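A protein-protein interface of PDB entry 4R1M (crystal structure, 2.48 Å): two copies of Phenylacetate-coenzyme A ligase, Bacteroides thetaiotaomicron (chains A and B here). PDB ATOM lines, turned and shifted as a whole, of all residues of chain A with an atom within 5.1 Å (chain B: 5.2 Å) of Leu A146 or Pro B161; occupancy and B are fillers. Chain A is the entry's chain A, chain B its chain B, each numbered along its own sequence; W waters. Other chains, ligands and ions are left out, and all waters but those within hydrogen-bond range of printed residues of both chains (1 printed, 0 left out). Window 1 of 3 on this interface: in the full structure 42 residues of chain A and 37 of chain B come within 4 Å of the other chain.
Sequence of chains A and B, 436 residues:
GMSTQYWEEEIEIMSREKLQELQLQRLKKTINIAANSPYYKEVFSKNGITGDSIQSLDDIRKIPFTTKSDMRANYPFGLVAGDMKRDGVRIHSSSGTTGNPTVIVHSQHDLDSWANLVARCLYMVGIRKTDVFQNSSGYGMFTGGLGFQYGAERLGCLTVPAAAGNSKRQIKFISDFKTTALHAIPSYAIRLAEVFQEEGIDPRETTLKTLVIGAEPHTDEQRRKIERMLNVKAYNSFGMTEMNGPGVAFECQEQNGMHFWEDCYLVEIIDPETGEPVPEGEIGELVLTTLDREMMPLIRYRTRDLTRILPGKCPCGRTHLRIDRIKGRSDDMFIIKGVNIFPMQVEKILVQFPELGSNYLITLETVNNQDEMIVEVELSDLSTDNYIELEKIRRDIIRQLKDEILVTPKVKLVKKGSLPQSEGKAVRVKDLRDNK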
ATOM      1  N   ARG A  90      -1.779  35.400   7.531  1.00  0.00           N
ATOM      2  CA  ARG A  90      -1.772  33.988   7.201  1.00  0.00           C
ATOM      3  C   ARG A  90      -0.972  33.672   5.966  1.00  0.00           C
ATOM      4  O   ARG A  90      -1.037  34.410   4.993  1.00  0.00           O
ATOM      5  CB  ARG A  90      -3.189  33.418   6.998  1.00  0.00           C
ATOM      6  CG  ARG A  90      -3.161  31.874   7.211  1.00  0.00           C
ATOM      7  CD  ARG A  90      -4.431  31.171   6.887  1.00  0.00           C
ATOM      8  NE  ARG A  90      -5.517  31.585   7.763  1.00  0.00           N
ATOM      9  CZ  ARG A  90      -6.790  31.412   7.472  1.00  0.00           C
ATOM     10  NH1 ARG A  90      -7.150  30.838   6.315  1.00  0.00           N
ATOM     11  NH2 ARG A  90      -7.721  31.812   8.318  1.00  0.00           N
ATOM     12  N   ILE A  91      -0.280  32.516   5.988  1.00  0.00           N
ATOM     13  CA  ILE A  91       0.451  31.929   4.862  1.00  0.00           C
ATOM     14  C   ILE A  91      -0.182  30.584   4.478  1.00  0.00           C
ATOM     15  O   ILE A  91      -0.268  29.724   5.332  1.00  0.00           O
ATOM     16  CB  ILE A  91       1.970  31.736   5.141  1.00  0.00           C
ATOM     17  CG1 ILE A  91       2.694  33.027   5.485  1.00  0.00           C
ATOM     18  CG2 ILE A  91       2.653  31.040   3.966  1.00  0.00           C
ATOM     19  CD1 ILE A  91       4.149  32.793   6.081  1.00  0.00           C
ATOM     20  N   HIS A  92      -0.593  30.392   3.213  1.00  0.00           N
ATOM     21  CA  HIS A  92      -1.055  29.111   2.674  1.00  0.00           C
ATOM     22  C   HIS A  92      -0.003  28.581   1.729  1.00  0.00           C
ATOM     23  O   HIS A  92       0.494  29.306   0.862  1.00  0.00           O
ATOM     24  CB  HIS A  92      -2.417  29.162   2.009  1.00  0.00           C
ATOM     25  CG  HIS A  92      -3.522  29.050   3.005  1.00  0.00           C
ATOM     26  ND1 HIS A  92      -3.829  27.841   3.602  1.00  0.00           N
ATOM     27  CD2 HIS A  92      -4.339  30.005   3.506  1.00  0.00           C
ATOM     28  CE1 HIS A  92      -4.835  28.089   4.423  1.00  0.00           C
ATOM     29  NE2 HIS A  92      -5.183  29.370   4.398  1.00  0.00           N
ATOM     30  N   TRP A 114     -12.240  36.891   1.357  1.00  0.00           N
ATOM     31  CA  TRP A 114     -12.309  35.463   1.072  1.00  0.00           C
ATOM     32  C   TRP A 114     -13.511  34.851   1.745  1.00  0.00           C
ATOM     33  O   TRP A 114     -14.278  34.169   1.071  1.00  0.00           O
ATOM     34  CB  TRP A 114     -11.021  34.768   1.530  1.00  0.00           C
ATOM     35  CG  TRP A 114     -10.932  33.278   1.317  1.00  0.00           C
ATOM     36  CD1 TRP A 114     -11.728  32.489   0.528  1.00  0.00           C
ATOM     37  CD2 TRP A 114      -9.897  32.422   1.828  1.00  0.00           C
ATOM     38  NE1 TRP A 114     -11.303  31.178   0.593  1.00  0.00           N
ATOM     39  CE2 TRP A 114     -10.172  31.112   1.369  1.00  0.00           C
ATOM     40  CE3 TRP A 114      -8.799  32.626   2.685  1.00  0.00           C
ATOM     41  CZ2 TRP A 114      -9.352  30.023   1.690  1.00  0.00           C
ATOM     42  CZ3 TRP A 114      -8.000  31.540   3.014  1.00  0.00           C
ATOM     43  CH2 TRP A 114      -8.273  30.260   2.510  1.00  0.00           C
ATOM     44  N   TYR A 139      -7.854  20.123   6.800  1.00  0.00           N
ATOM     45  CA  TYR A 139      -7.605  21.463   7.350  1.00  0.00           C
ATOM     46  C   TYR A 139      -6.091  21.755   7.207  1.00  0.00           C
ATOM     47  O   TYR A 139      -5.510  21.367   6.183  1.00  0.00           O
ATOM     48  CB  TYR A 139      -8.141  21.582   8.800  1.00  0.00           C
ATOM     49  CG  TYR A 139      -9.627  21.883   8.860  1.00  0.00           C
ATOM     50  CD1 TYR A 139     -10.571  20.962   8.387  1.00  0.00           C
ATOM     51  CD2 TYR A 139     -10.093  23.093   9.367  1.00  0.00           C
ATOM     52  CE1 TYR A 139     -11.933  21.270   8.356  1.00  0.00           C
ATOM     53  CE2 TYR A 139     -11.457  23.391   9.386  1.00  0.00           C
ATOM     54  CZ  TYR A 139     -12.371  22.486   8.857  1.00  0.00           C
ATOM     55  OH  TYR A 139     -13.710  22.791   8.849  1.00  0.00           O
ATOM     56  N   GLY A 140      -5.485  22.486   8.150  1.00  0.00           N
ATOM     57  CA  GLY A 140      -4.075  22.856   8.047  1.00  0.00           C
ATOM     58  C   GLY A 140      -3.797  23.740   6.836  1.00  0.00           C
ATOM     59  O   GLY A 140      -4.513  24.732   6.623  1.00  0.00           O
ATOM     60  N   MET A 141      -2.806  23.352   5.995  1.00  0.00           N
ATOM     61  CA  MET A 141      -2.422  24.140   4.820  1.00  0.00           C
ATOM     62  C   MET A 141      -3.478  24.053   3.666  1.00  0.00           C
ATOM     63  O   MET A 141      -3.408  24.866   2.732  1.00  0.00           O
ATOM     64  CB  MET A 141      -1.026  23.734   4.291  1.00  0.00           C
ATOM     65  CG  MET A 141       0.130  24.294   5.146  1.00  0.00           C
ATOM     66  SD  MET A 141       0.040  26.276   5.285  1.00  0.00           S
ATOM     67  CE  MET A 141       1.584  26.627   6.172  1.00  0.00           C
ATOM     68  N   PHE A 142      -4.458  23.115   3.756  1.00  0.00           N
ATOM     69  CA  PHE A 142      -5.540  22.974   2.769  1.00  0.00           C
ATOM     70  C   PHE A 142      -6.496  24.159   2.904  1.00  0.00           C
ATOM     71  O   PHE A 142      -7.028  24.440   3.992  1.00  0.00           O
ATOM     72  CB  PHE A 142      -6.293  21.633   2.897  1.00  0.00           C
ATOM     73  CG  PHE A 142      -5.456  20.410   2.615  1.00  0.00           C
ATOM     74  CD1 PHE A 142      -5.135  20.053   1.308  1.00  0.00           C
ATOM     75  CD2 PHE A 142      -4.985  19.612   3.653  1.00  0.00           C
ATOM     76  CE1 PHE A 142      -4.342  18.930   1.047  1.00  0.00           C
ATOM     77  CE2 PHE A 142      -4.194  18.485   3.393  1.00  0.00           C
ATOM     78  CZ  PHE A 142      -3.888  18.144   2.093  1.00  0.00           C
ATOM     79  N   THR A 143      -6.672  24.877   1.798  1.00  0.00           N
ATOM     80  CA  THR A 143      -7.483  26.079   1.767  1.00  0.00           C
ATOM     81  C   THR A 143      -8.974  25.714   1.876  1.00  0.00           C
ATOM     82  O   THR A 143      -9.731  26.565   2.345  1.00  0.00           O
ATOM     83  CB  THR A 143      -7.178  26.927   0.534  1.00  0.00           C
ATOM     84  OG1 THR A 143      -7.350  26.168  -0.681  1.00  0.00           O
ATOM     85  CG2 THR A 143      -5.802  27.513   0.604  1.00  0.00           C
ATOM     86  N   GLY A 144      -9.361  24.472   1.518  1.00  0.00           N
ATOM     87  CA  GLY A 144     -10.736  23.982   1.636  1.00  0.00           C
ATOM     88  C   GLY A 144     -11.200  23.925   3.087  1.00  0.00           C
ATOM     89  O   GLY A 144     -12.389  24.114   3.371  1.00  0.00           O
ATOM     90  N   GLY A 145     -10.236  23.703   4.003  1.00  0.00           N
ATOM     91  CA  GLY A 145     -10.457  23.593   5.432  1.00  0.00           C
ATOM     92  C   GLY A 145     -10.855  24.918   6.019  1.00  0.00           C
ATOM     93  O   GLY A 145     -12.046  25.193   6.192  1.00  0.00           O
ATOM     94  N   LEU A 146      -9.869  25.784   6.231  1.00  0.00           N
ATOM     95  CA  LEU A 146     -10.086  27.112   6.825  1.00  0.00           C
ATOM     96  C   LEU A 146     -10.992  28.003   5.930  1.00  0.00           C
ATOM     97  O   LEU A 146     -11.742  28.819   6.461  1.00  0.00           O
ATOM     98  CB  LEU A 146      -8.734  27.822   7.105  1.00  0.00           C
ATOM     99  CG  LEU A 146      -7.835  27.139   8.178  1.00  0.00           C
ATOM    100  CD1 LEU A 146      -6.408  27.686   8.160  1.00  0.00           C
ATOM    101  CD2 LEU A 146      -8.428  27.267   9.585  1.00  0.00           C
ATOM    102  N   GLY A 147     -10.976  27.801   4.628  1.00  0.00           N
ATOM    103  CA  GLY A 147     -11.830  28.537   3.695  1.00  0.00           C
ATOM    104  C   GLY A 147     -13.316  28.325   3.880  1.00  0.00           C
ATOM    105  O   GLY A 147     -14.067  29.300   3.984  1.00  0.00           O
ATOM    106  N   PHE A 148     -13.768  27.057   3.925  1.00  0.00           N
ATOM    107  CA  PHE A 148     -15.184  26.784   4.196  1.00  0.00           C
ATOM    108  C   PHE A 148     -15.525  27.046   5.659  1.00  0.00           C
ATOM    109  O   PHE A 148     -16.631  27.518   5.925  1.00  0.00           O
ATOM    110  CB  PHE A 148     -15.574  25.357   3.824  1.00  0.00           C
ATOM    111  CG  PHE A 148     -15.951  25.251   2.376  1.00  0.00           C
ATOM    112  CD1 PHE A 148     -17.127  25.814   1.910  1.00  0.00           C
ATOM    113  CD2 PHE A 148     -15.149  24.561   1.482  1.00  0.00           C
ATOM    114  CE1 PHE A 148     -17.454  25.754   0.564  1.00  0.00           C
ATOM    115  CE2 PHE A 148     -15.506  24.460   0.138  1.00  0.00           C
ATOM    116  CZ  PHE A 148     -16.652  25.059  -0.309  1.00  0.00           C
ATOM    117  N   GLN A 149     -14.574  26.781   6.594  1.00  0.00           N
ATOM    118  CA  GLN A 149     -14.778  27.018   8.021  1.00  0.00           C
ATOM    119  C   GLN A 149     -15.132  28.495   8.288  1.00  0.00           C
ATOM    120  O   GLN A 149     -16.114  28.761   8.964  1.00  0.00           O
ATOM    121  CB  GLN A 149     -13.526  26.611   8.832  1.00  0.00           C
ATOM    122  CG  GLN A 149     -13.689  26.693  10.343  1.00  0.00           C
ATOM    123  CD  GLN A 149     -14.820  25.810  10.808  1.00  0.00           C
ATOM    124  OE1 GLN A 149     -14.887  24.620  10.467  1.00  0.00           O
ATOM    125  NE2 GLN A 149     -15.756  26.387  11.558  1.00  0.00           N
ATOM    126  N   TYR A 150     -14.360  29.435   7.728  1.00  0.00           N
ATOM    127  CA  TYR A 150     -14.572  30.884   7.909  1.00  0.00           C
ATOM    128  C   TYR A 150     -15.819  31.364   7.153  1.00  0.00           C
ATOM    129  O   TYR A 150     -16.577  32.141   7.727  1.00  0.00           O
ATOM    130  CB  TYR A 150     -13.339  31.688   7.464  1.00  0.00           C
ATOM    131  CG  TYR A 150     -12.237  31.758   8.504  1.00  0.00           C
ATOM    132  CD1 TYR A 150     -11.752  30.601   9.121  1.00  0.00           C
ATOM    133  CD2 TYR A 150     -11.580  32.955   8.768  1.00  0.00           C
ATOM    134  CE1 TYR A 150     -10.692  30.648  10.031  1.00  0.00           C
ATOM    135  CE2 TYR A 150     -10.524  33.018   9.690  1.00  0.00           C
ATOM    136  CZ  TYR A 150     -10.095  31.863  10.331  1.00  0.00           C
ATOM    137  OH  TYR A 150      -9.052  31.910  11.237  1.00  0.00           O
ATOM    138  N   GLY A 151     -16.021  30.904   5.906  1.00  0.00           N
ATOM    139  CA  GLY A 151     -17.192  31.255   5.115  1.00  0.00           C
ATOM    140  C   GLY A 151     -18.507  30.840   5.759  1.00  0.00           C
ATOM    141  O   GLY A 151     -19.446  31.646   5.847  1.00  0.00           O
ATOM    142  N   ASN B 135       1.486  26.647  14.026  1.00  0.00           N
ATOM    143  CA  ASN B 135       0.693  25.768  14.868  1.00  0.00           C
ATOM    144  C   ASN B 135       0.794  24.297  14.368  1.00  0.00           C
ATOM    145  O   ASN B 135       0.155  23.923  13.371  1.00  0.00           O
ATOM    146  CB  ASN B 135      -0.750  26.252  14.902  1.00  0.00           C
ATOM    147  CG  ASN B 135      -1.635  25.522  15.873  1.00  0.00           C
ATOM    148  OD1 ASN B 135      -1.178  24.897  16.853  1.00  0.00           O
ATOM    149  ND2 ASN B 135      -2.939  25.642  15.640  1.00  0.00           N
ATOM    150  N   TYR B 139      -5.824  19.963  13.490  1.00  0.00           N
ATOM    151  CA  TYR B 139      -6.952  20.877  13.248  1.00  0.00           C
ATOM    152  C   TYR B 139      -8.264  20.038  13.281  1.00  0.00           C
ATOM    153  O   TYR B 139      -8.355  19.124  14.115  1.00  0.00           O
ATOM    154  CB  TYR B 139      -6.753  21.683  11.942  1.00  0.00           C
ATOM    155  CG  TYR B 139      -5.883  22.907  12.146  1.00  0.00           C
ATOM    156  CD1 TYR B 139      -4.531  22.783  12.465  1.00  0.00           C
ATOM    157  CD2 TYR B 139      -6.393  24.190  11.960  1.00  0.00           C
ATOM    158  CE1 TYR B 139      -3.725  23.904  12.662  1.00  0.00           C
ATOM    159  CE2 TYR B 139      -5.588  25.323  12.115  1.00  0.00           C
ATOM    160  CZ  TYR B 139      -4.258  25.176  12.494  1.00  0.00           C
ATOM    161  OH  TYR B 139      -3.461  26.277  12.716  1.00  0.00           O
ATOM    162  N   LEU B 146      -8.046  25.116  15.636  1.00  0.00           N
ATOM    163  CA  LEU B 146      -8.790  26.351  15.399  1.00  0.00           C
ATOM    164  C   LEU B 146      -8.657  27.350  16.590  1.00  0.00           C
ATOM    165  O   LEU B 146      -8.724  28.560  16.360  1.00  0.00           O
ATOM    166  CB  LEU B 146     -10.275  26.050  15.116  1.00  0.00           C
ATOM    167  CG  LEU B 146     -10.607  25.275  13.806  1.00  0.00           C
ATOM    168  CD1 LEU B 146     -12.010  24.706  13.831  1.00  0.00           C
ATOM    169  CD2 LEU B 146     -10.413  26.131  12.572  1.00  0.00           C
ATOM    170  N   GLN B 149      -5.298  29.095  16.054  1.00  0.00           N
ATOM    171  CA  GLN B 149      -5.419  29.749  14.756  1.00  0.00           C
ATOM    172  C   GLN B 149      -6.170  31.068  14.900  1.00  0.00           C
ATOM    173  O   GLN B 149      -5.666  32.085  14.441  1.00  0.00           O
ATOM    174  CB  GLN B 149      -6.122  28.812  13.734  1.00  0.00           C
ATOM    175  CG  GLN B 149      -6.190  29.367  12.315  1.00  0.00           C
ATOM    176  CD  GLN B 149      -4.814  29.641  11.780  1.00  0.00           C
ATOM    177  OE1 GLN B 149      -3.928  28.779  11.815  1.00  0.00           O
ATOM    178  NE2 GLN B 149      -4.598  30.854  11.306  1.00  0.00           N
ATOM    179  N   THR B 159       0.412  33.782  10.687  1.00  0.00           N
ATOM    180  CA  THR B 159       0.227  32.388  11.071  1.00  0.00           C
ATOM    181  C   THR B 159       0.542  31.430   9.922  1.00  0.00           C
ATOM    182  O   THR B 159       0.301  31.719   8.745  1.00  0.00           O
ATOM    183  CB  THR B 159      -1.191  32.140  11.580  1.00  0.00           C
ATOM    184  OG1 THR B 159      -2.119  32.288  10.479  1.00  0.00           O
ATOM    185  CG2 THR B 159      -1.545  33.052  12.765  1.00  0.00           C
ATOM    186  N   VAL B 160       1.089  30.271  10.313  1.00  0.00           N
ATOM    187  CA  VAL B 160       1.489  29.156   9.472  1.00  0.00           C
ATOM    188  C   VAL B 160       0.666  27.943   9.942  1.00  0.00           C
ATOM    189  O   VAL B 160       1.043  27.300  10.923  1.00  0.00           O
ATOM    190  CB  VAL B 160       3.027  28.953   9.557  1.00  0.00           C
ATOM    191  CG1 VAL B 160       3.491  27.797   8.687  1.00  0.00           C
ATOM    192  CG2 VAL B 160       3.772  30.215   9.189  1.00  0.00           C
ATOM    193  N   PRO B 161      -0.516  27.666   9.351  1.00  0.00           N
ATOM    194  CA  PRO B 161      -1.343  26.540   9.868  1.00  0.00           C
ATOM    195  C   PRO B 161      -0.800  25.165   9.423  1.00  0.00           C
ATOM    196  O   PRO B 161      -1.456  24.438   8.698  1.00  0.00           O
ATOM    197  CB  PRO B 161      -2.733  26.820   9.268  1.00  0.00           C
ATOM    198  CG  PRO B 161      -2.456  27.605   8.000  1.00  0.00           C
ATOM    199  CD  PRO B 161      -1.165  28.363   8.214  1.00  0.00           C
ATOM    200  N   ALA B 162       0.389  24.808   9.881  1.00  0.00           N
ATOM    201  CA  ALA B 162       1.118  23.571   9.541  1.00  0.00           C
ATOM    202  C   ALA B 162       0.309  22.285   9.842  1.00  0.00           C
ATOM    203  O   ALA B 162       0.374  21.313   9.078  1.00  0.00           O
ATOM    204  CB  ALA B 162       2.435  23.525  10.324  1.00  0.00           C
ATOM    205  N   ALA B 163      -0.426  22.294  10.963  1.00  0.00           N
ATOM    206  CA  ALA B 163      -1.181  21.170  11.530  1.00  0.00           C
ATOM    207  C   ALA B 163      -0.189  20.055  11.990  1.00  0.00           C
ATOM    208  O   ALA B 163       1.041  20.278  11.990  1.00  0.00           O
ATOM    209  CB  ALA B 163      -2.229  20.630  10.551  1.00  0.00           C
HETATM  210  O   HOH W   1      -1.278  20.927   6.693  1.00  0.00           O
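The backbone NH of Ile A91 sits at hydrogen-bond distance from the backbone carbonyl oxygen of Thr B159. The backbone NH of Met A141 sits at hydrogen-bond distance from the backbone carbonyl oxygen of Pro B161, at 3.2 Å.
Water W1 lies within hydrogen-bond range of the backbone carbonyl oxygen of Ala B162 and the backbone NH of Met A141.
Tyr B139 touches its own counterpart, Tyr A139. Leu A146 touches its own counterpart, Leu B146. 3 positions are printed for both chains.
Among the printed residues, merely in contact across the chains: Arg A90 with Gln B149, Arg A90 with Thr B159, Ile A91 with Pro B161, Tyr A139 with Tyr B139, Gly A140 with Pro B161, Gly A140 with Ala B163, Met A141 with Val B160, Leu A146 with Leu B146, Leu A146 with Pro B161 and Tyr A150 with Gln B149.
Of the 9 printed residues of chain B, 7 touch a printed residue of chain A. Of the 17 printed residues of chain A, 7 touch a printed residue of chain B. Among the printed residues, no Asp or Glu carboxylate lies within 4 Å of a Lys or Arg side-chain nitrogen of the other chain.
The backbone NH (N) of Asn B135 sits at hydrogen-bond distance from the backbone carbonyl oxygen (O) of Val B160 (3.2 Å). The backbone carbonyl oxygen of Asn B135 lies within hydrogen-bond range of the backbone NH of Ala B163, 3.0 Å away. A ring nitrogen (ND1) of His A92 is in hydrogen-bond range of the backbone carbonyl oxygen (O) of Met A141. OH of Tyr B139 is in hydrogen-bond range of OE1 of Gln B149, at 2.7 Å. The guanidinium group (NH1) of Arg A90 lies within hydrogen-bond range of a ring nitrogen (NE2) of His A92 (3.1 Å). The side-chain amide nitrogen (ND2) of Asn B135 sits at hydrogen-bond distance from the side-chain hydroxyl (OH) of Tyr B139, at 3.0 Å.
Leu A146 touches just these residues of chain B: Leu B146 (3.8 Å) and Pro B161 (3.9 Å). Of chain A, only Ile A91, Gly A140, Met A141 and Leu A146 come within 4 Å of Pro B161. Of the printed residues of chain A, Tyr B139 touches Tyr A139 (3.4 Å). Of the printed residues of chain A, Gln B149 touches Arg A90 and Tyr A150. Of the printed residues of chain A, Thr B159 touches Arg A90 and Ile A91. Printed residues of chain A within 4 Å of Ala B163: Gly A140. Printed residues of chain B within 4 Å of Ile A91: Thr B159 and Pro B161. Thr A143 touches none of the printed residues of chain B.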
